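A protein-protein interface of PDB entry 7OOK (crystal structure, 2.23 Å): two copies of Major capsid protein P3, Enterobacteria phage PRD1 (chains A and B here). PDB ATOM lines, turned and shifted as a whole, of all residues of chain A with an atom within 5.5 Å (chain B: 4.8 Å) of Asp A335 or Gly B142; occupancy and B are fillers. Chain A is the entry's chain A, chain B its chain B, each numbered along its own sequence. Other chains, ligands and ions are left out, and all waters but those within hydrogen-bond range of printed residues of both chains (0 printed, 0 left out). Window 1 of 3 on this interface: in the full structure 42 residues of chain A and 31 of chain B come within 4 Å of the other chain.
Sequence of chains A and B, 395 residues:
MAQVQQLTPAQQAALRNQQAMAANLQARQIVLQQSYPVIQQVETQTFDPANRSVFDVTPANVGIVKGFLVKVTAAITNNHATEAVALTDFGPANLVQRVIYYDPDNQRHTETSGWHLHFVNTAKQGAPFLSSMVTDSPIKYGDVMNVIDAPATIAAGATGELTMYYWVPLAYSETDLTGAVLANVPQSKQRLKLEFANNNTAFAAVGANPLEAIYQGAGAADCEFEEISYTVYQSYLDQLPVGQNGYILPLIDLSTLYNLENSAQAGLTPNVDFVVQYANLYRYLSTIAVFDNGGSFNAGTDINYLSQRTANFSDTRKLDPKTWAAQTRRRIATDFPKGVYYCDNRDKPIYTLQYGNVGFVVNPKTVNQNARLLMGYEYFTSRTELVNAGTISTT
Of the printed residues of chain B, Ala A325 touches Met B145.
Printed residues of chain A within 4 Å of Met B145: Ala A325 and Asp A335.
Of the printed residues of chain B, Phe A336 touches Tyr B141 and Val B144.
Of the printed residues of chain A, Lys B140 touches Pro A337.
Of the printed residues of chain B, Arg A329 touches Ser B132 (3.6 Å), Asp B143 (3.2 Å), Asn B146 (3.4 Å) and Val B147 (3.3 Å).
Thr A328 touches none of the printed residues of chain B.
Ile A332 touches none of the printed residues of chain B.
The nearest residue of chain B that does not touch Asp A335 is Asn B146 (4.1 Å).
Printed residues of chain A that touch a printed residue of chain B: Ala A325, Arg A329, Ala A333, Thr A334, Asp A335, Phe A336 and Pro A337.
Hydrophobic or aromatic side chains of chain A that line the printed part of chain B: Ala A325, Phe A336 and Pro A337.
Hydrophobic or aromatic side chains of chain B within 4 Å of the printed part of chain A: Tyr B141, Val B144, Met B145 and Val B147.
Among the printed residues, 16 pairs touch across the chains.
Among the printed residues, Asp or Glu carboxylates within 4 Å of a Lys or Arg side-chain nitrogen of the other chain: Arg A329 with Asp B143.
OG of Ser B132 lies close to O of Gly B142 (3.1 Å).
The backbone NH (N) of Asp B143 sits at hydrogen-bond distance from the side-chain hydroxyl (OG) of Ser B132.
The side-chain carboxylate of Asp B143 lies close to the side-chain amide oxygen of Asn B146 (3.1 Å).
The guanidinium group (NH2) of Arg A329 lies within salt-bridge range of the side-chain carboxylate (OD2) of Asp A335 (2.7 Å).
The side-chain hydroxyl (OG1) of Thr A334 is in hydrogen-bond range of the side-chain hydroxyl (OG) of Ser B132 (2.7 Å).
The side-chain hydroxyl (OG1) of Thr A334 is in hydrogen-bond range of the backbone NH (N) of Gly B142.
The backbone NH (N) of Asp A335 lies close to the backbone carbonyl oxygen (O) of Gly B142.
OD1 of Asp B143 lies within salt-bridge range of NH2 of Arg A329 (3.2 Å).
The side-chain carboxylate of Asp A335 is in hydrogen-bond range of the backbone NH of Val B144 (2.9 Å).
The backbone NH (N) of Met B145 lies within hydrogen-bond range of the side-chain carboxylate (OD2) of Asp A335, at 2.8 Å.
The guanidinium group of Arg A329 sits close to the backbone NH of Asn B146.
The guanidinium group of Arg A329 sits close to the backbone NH of Val B147 (3.5 Å).
No position is printed for both chains.
Among the printed residues, pairs that only touch across the chains: Ala A325 with Met B145 (3.6 Å), Arg A329 with Ser B132 (3.6 Å), Ala A333 with Ser B132 (3.5 Å), Asp A335 with Tyr B141 (3.4 Å), Asp A335 with Asp B143 (3.8 Å), Phe A336 with Tyr B141 (3.5 Å), Phe A336 with Val B144 (3.5 Å) and Pro A337 with Lys B140 (3.5 Å).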
ATOM      1  N   ALA A 325      30.430   3.189 -24.320  1.00  0.00           N
ATOM      2  CA  ALA A 325      29.056   3.170 -24.809  1.00  0.00           C
ATOM      3  C   ALA A 325      28.571   1.752 -25.073  1.00  0.00           C
ATOM      4  O   ALA A 325      27.376   1.469 -24.936  1.00  0.00           O
ATOM      5  CB  ALA A 325      28.938   4.008 -26.085  1.00  0.00           C
ATOM      6  N   THR A 328      27.126   0.389 -22.020  1.00  0.00           N
ATOM      7  CA  THR A 328      25.833   1.025 -21.786  1.00  0.00           C
ATOM      8  C   THR A 328      24.756   0.435 -22.692  1.00  0.00           C
ATOM      9  O   THR A 328      23.599   0.303 -22.279  1.00  0.00           O
ATOM     10  CB  THR A 328      25.947   2.537 -21.998  1.00  0.00           C
ATOM     11  OG1 THR A 328      26.781   3.100 -20.979  1.00  0.00           O
ATOM     12  CG2 THR A 328      24.583   3.209 -21.948  1.00  0.00           C
ATOM     13  N   ARG A 329      25.115   0.078 -23.928  1.00  0.00           N
ATOM     14  CA  ARG A 329      24.146  -0.552 -24.818  1.00  0.00           C
ATOM     15  C   ARG A 329      23.665  -1.887 -24.266  1.00  0.00           C
ATOM     16  O   ARG A 329      22.533  -2.299 -24.538  1.00  0.00           O
ATOM     17  CB  ARG A 329      24.745  -0.734 -26.209  1.00  0.00           C
ATOM     18  CG  ARG A 329      24.832   0.550 -27.002  1.00  0.00           C
ATOM     19  CD  ARG A 329      25.015   0.265 -28.476  1.00  0.00           C
ATOM     20  NE  ARG A 329      25.114   1.491 -29.257  1.00  0.00           N
ATOM     21  CZ  ARG A 329      25.037   1.543 -30.578  1.00  0.00           C
ATOM     22  NH1 ARG A 329      24.837   0.453 -31.302  1.00  0.00           N
ATOM     23  NH2 ARG A 329      25.163   2.718 -31.189  1.00  0.00           N
ATOM     24  N   ILE A 332      20.813  -0.489 -21.542  1.00  0.00           N
ATOM     25  CA  ILE A 332      19.566   0.172 -21.915  1.00  0.00           C
ATOM     26  C   ILE A 332      19.223  -0.029 -23.387  1.00  0.00           C
ATOM     27  O   ILE A 332      18.318   0.626 -23.917  1.00  0.00           O
ATOM     28  CB  ILE A 332      19.624   1.680 -21.587  1.00  0.00           C
ATOM     29  CG1 ILE A 332      20.746   2.359 -22.374  1.00  0.00           C
ATOM     30  CG2 ILE A 332      19.817   1.891 -20.090  1.00  0.00           C
ATOM     31  CD1 ILE A 332      20.578   3.875 -22.486  1.00  0.00           C
ATOM     32  N   ALA A 333      19.940  -0.927 -24.058  1.00  0.00           N
ATOM     33  CA  ALA A 333      19.640  -1.328 -25.430  1.00  0.00           C
ATOM     34  C   ALA A 333      19.763  -0.179 -26.426  1.00  0.00           C
ATOM     35  O   ALA A 333      19.197  -0.243 -27.523  1.00  0.00           O
ATOM     36  CB  ALA A 333      18.240  -1.949 -25.525  1.00  0.00           C
ATOM     37  N   THR A 334      20.499   0.872 -26.077  1.00  0.00           N
ATOM     38  CA  THR A 334      20.721   2.007 -26.969  1.00  0.00           C
ATOM     39  C   THR A 334      21.755   2.916 -26.311  1.00  0.00           C
ATOM     40  O   THR A 334      22.292   2.605 -25.242  1.00  0.00           O
ATOM     41  CB  THR A 334      19.413   2.747 -27.268  1.00  0.00           C
ATOM     42  OG1 THR A 334      19.634   3.743 -28.277  1.00  0.00           O
ATOM     43  CG2 THR A 334      18.856   3.413 -26.011  1.00  0.00           C
ATOM     44  N   ASP A 335      22.042   4.037 -26.967  1.00  0.00           N
ATOM     45  CA  ASP A 335      22.953   5.039 -26.437  1.00  0.00           C
ATOM     46  C   ASP A 335      22.161   6.141 -25.746  1.00  0.00           C
ATOM     47  O   ASP A 335      21.083   6.527 -26.209  1.00  0.00           O
ATOM     48  CB  ASP A 335      23.805   5.680 -27.535  1.00  0.00           C
ATOM     49  CG  ASP A 335      24.679   4.686 -28.267  1.00  0.00           C
ATOM     50  OD1 ASP A 335      25.268   3.800 -27.616  1.00  0.00           O
ATOM     51  OD2 ASP A 335      24.775   4.806 -29.506  1.00  0.00           O
ATOM     52  N   PHE A 336      22.707   6.655 -24.648  1.00  0.00           N
ATOM     53  CA  PHE A 336      22.231   7.917 -24.114  1.00  0.00           C
ATOM     54  C   PHE A 336      22.546   9.037 -25.108  1.00  0.00           C
ATOM     55  O   PHE A 336      23.385   8.876 -25.996  1.00  0.00           O
ATOM     56  CB  PHE A 336      22.875   8.205 -22.763  1.00  0.00           C
ATOM     57  CG  PHE A 336      22.254   7.453 -21.620  1.00  0.00           C
ATOM     58  CD1 PHE A 336      21.031   7.838 -21.100  1.00  0.00           C
ATOM     59  CD2 PHE A 336      22.900   6.369 -21.055  1.00  0.00           C
ATOM     60  CE1 PHE A 336      20.460   7.152 -20.051  1.00  0.00           C
ATOM     61  CE2 PHE A 336      22.335   5.681 -20.002  1.00  0.00           C
ATOM     62  CZ  PHE A 336      21.114   6.071 -19.499  1.00  0.00           C
ATOM     63  N   PRO A 337      21.872  10.179 -24.989  1.00  0.00           N
ATOM     64  CA  PRO A 337      22.136  11.290 -25.913  1.00  0.00           C
ATOM     65  C   PRO A 337      23.598  11.721 -25.898  1.00  0.00           C
ATOM     66  O   PRO A 337      24.366  11.390 -24.992  1.00  0.00           O
ATOM     67  CB  PRO A 337      21.219  12.410 -25.397  1.00  0.00           C
ATOM     68  CG  PRO A 337      20.130  11.692 -24.652  1.00  0.00           C
ATOM     69  CD  PRO A 337      20.784  10.484 -24.042  1.00  0.00           C
ATOM     70  N   SER B 132      21.478  -0.811 -31.178  1.00  0.00           N
ATOM     71  CA  SER B 132      20.653   0.269 -30.652  1.00  0.00           C
ATOM     72  C   SER B 132      19.218   0.062 -31.124  1.00  0.00           C
ATOM     73  O   SER B 132      18.943   0.089 -32.328  1.00  0.00           O
ATOM     74  CB  SER B 132      21.179   1.634 -31.093  1.00  0.00           C
ATOM     75  OG  SER B 132      20.334   2.673 -30.625  1.00  0.00           O
ATOM     76  N   LYS B 140      16.672  12.250 -27.373  1.00  0.00           N
ATOM     77  CA  LYS B 140      17.493  11.816 -28.502  1.00  0.00           C
ATOM     78  C   LYS B 140      18.412  10.656 -28.111  1.00  0.00           C
ATOM     79  O   LYS B 140      19.635  10.702 -28.249  1.00  0.00           O
ATOM     80  CB  LYS B 140      18.274  12.996 -29.067  1.00  0.00           C
ATOM     81  CG  LYS B 140      17.354  14.090 -29.600  1.00  0.00           C
ATOM     82  CD  LYS B 140      17.980  14.887 -30.731  1.00  0.00           C
ATOM     83  CE  LYS B 140      16.988  15.904 -31.283  1.00  0.00           C
ATOM     84  NZ  LYS B 140      17.548  16.663 -32.438  1.00  0.00           N
ATOM     85  N   TYR B 141      17.781   9.594 -27.613  1.00  0.00           N
ATOM     86  CA  TYR B 141      18.411   8.288 -27.600  1.00  0.00           C
ATOM     87  C   TYR B 141      18.603   7.803 -29.035  1.00  0.00           C
ATOM     88  O   TYR B 141      18.068   8.373 -29.992  1.00  0.00           O
ATOM     89  CB  TYR B 141      17.561   7.269 -26.842  1.00  0.00           C
ATOM     90  CG  TYR B 141      17.347   7.569 -25.381  1.00  0.00           C
ATOM     91  CD1 TYR B 141      18.326   7.272 -24.443  1.00  0.00           C
ATOM     92  CD2 TYR B 141      16.157   8.131 -24.934  1.00  0.00           C
ATOM     93  CE1 TYR B 141      18.133   7.538 -23.105  1.00  0.00           C
ATOM     94  CE2 TYR B 141      15.952   8.397 -23.597  1.00  0.00           C
ATOM     95  CZ  TYR B 141      16.946   8.100 -22.687  1.00  0.00           C
ATOM     96  OH  TYR B 141      16.749   8.366 -21.353  1.00  0.00           O
ATOM     97  N   GLY B 142      19.358   6.722 -29.176  1.00  0.00           N
ATOM     98  CA  GLY B 142      19.451   6.050 -30.455  1.00  0.00           C
ATOM     99  C   GLY B 142      20.865   5.673 -30.820  1.00  0.00           C
ATOM    100  O   GLY B 142      21.693   5.399 -29.946  1.00  0.00           O
ATOM    101  N   ASP B 143      21.145   5.645 -32.121  1.00  0.00           N
ATOM    102  CA  ASP B 143      22.475   5.332 -32.631  1.00  0.00           C
ATOM    103  C   ASP B 143      23.306   6.607 -32.547  1.00  0.00           C
ATOM    104  O   ASP B 143      23.481   7.350 -33.515  1.00  0.00           O
ATOM    105  CB  ASP B 143      22.391   4.786 -34.049  1.00  0.00           C
ATOM    106  CG  ASP B 143      23.740   4.367 -34.591  1.00  0.00           C
ATOM    107  OD1 ASP B 143      24.732   4.418 -33.832  1.00  0.00           O
ATOM    108  OD2 ASP B 143      23.804   3.990 -35.779  1.00  0.00           O
ATOM    109  N   VAL B 144      23.812   6.866 -31.346  1.00  0.00           N
ATOM    110  CA  VAL B 144      24.636   8.040 -31.094  1.00  0.00           C
ATOM    111  C   VAL B 144      26.110   7.732 -31.303  1.00  0.00           C
ATOM    112  O   VAL B 144      26.834   8.526 -31.907  1.00  0.00           O
ATOM    113  CB  VAL B 144      24.378   8.558 -29.663  1.00  0.00           C
ATOM    114  CG1 VAL B 144      25.322   9.703 -29.327  1.00  0.00           C
ATOM    115  CG2 VAL B 144      22.938   8.989 -29.504  1.00  0.00           C
ATOM    116  N   MET B 145      26.571   6.587 -30.803  1.00  0.00           N
ATOM    117  CA  MET B 145      27.994   6.291 -30.716  1.00  0.00           C
ATOM    118  C   MET B 145      28.476   5.296 -31.759  1.00  0.00           C
ATOM    119  O   MET B 145      29.676   5.022 -31.817  1.00  0.00           O
ATOM    120  CB  MET B 145      28.329   5.762 -29.320  1.00  0.00           C
ATOM    121  CG  MET B 145      28.119   6.776 -28.213  1.00  0.00           C
ATOM    122  SD  MET B 145      29.299   8.145 -28.280  1.00  0.00           S
ATOM    123  CE  MET B 145      30.833   7.295 -27.910  1.00  0.00           C
ATOM    124  N   ASN B 146      27.575   4.736 -32.565  1.00  0.00           N
ATOM    125  CA  ASN B 146      27.939   3.834 -33.657  1.00  0.00           C
ATOM    126  C   ASN B 146      28.856   2.710 -33.184  1.00  0.00           C
ATOM    127  O   ASN B 146      29.897   2.430 -33.782  1.00  0.00           O
ATOM    128  CB  ASN B 146      28.585   4.613 -34.802  1.00  0.00           C
ATOM    129  CG  ASN B 146      27.630   5.592 -35.446  1.00  0.00           C
ATOM    130  OD1 ASN B 146      26.681   5.196 -36.121  1.00  0.00           O
ATOM    131  ND2 ASN B 146      27.870   6.879 -35.234  1.00  0.00           N
ATOM    132  N   VAL B 147      28.439   2.037 -32.108  1.00  0.00           N
ATOM    133  CA  VAL B 147      29.270   0.991 -31.508  1.00  0.00           C
ATOM    134  C   VAL B 147      29.576  -0.096 -32.530  1.00  0.00           C
ATOM    135  O   VAL B 147      30.734  -0.500 -32.704  1.00  0.00           O
ATOM    136  CB  VAL B 147      28.584   0.419 -30.255  1.00  0.00           C
ATOM    137  CG1 VAL B 147      29.368  -0.763 -29.693  1.00  0.00           C
ATOM    138  CG2 VAL B 147      28.437   1.506 -29.207  1.00  0.00           C
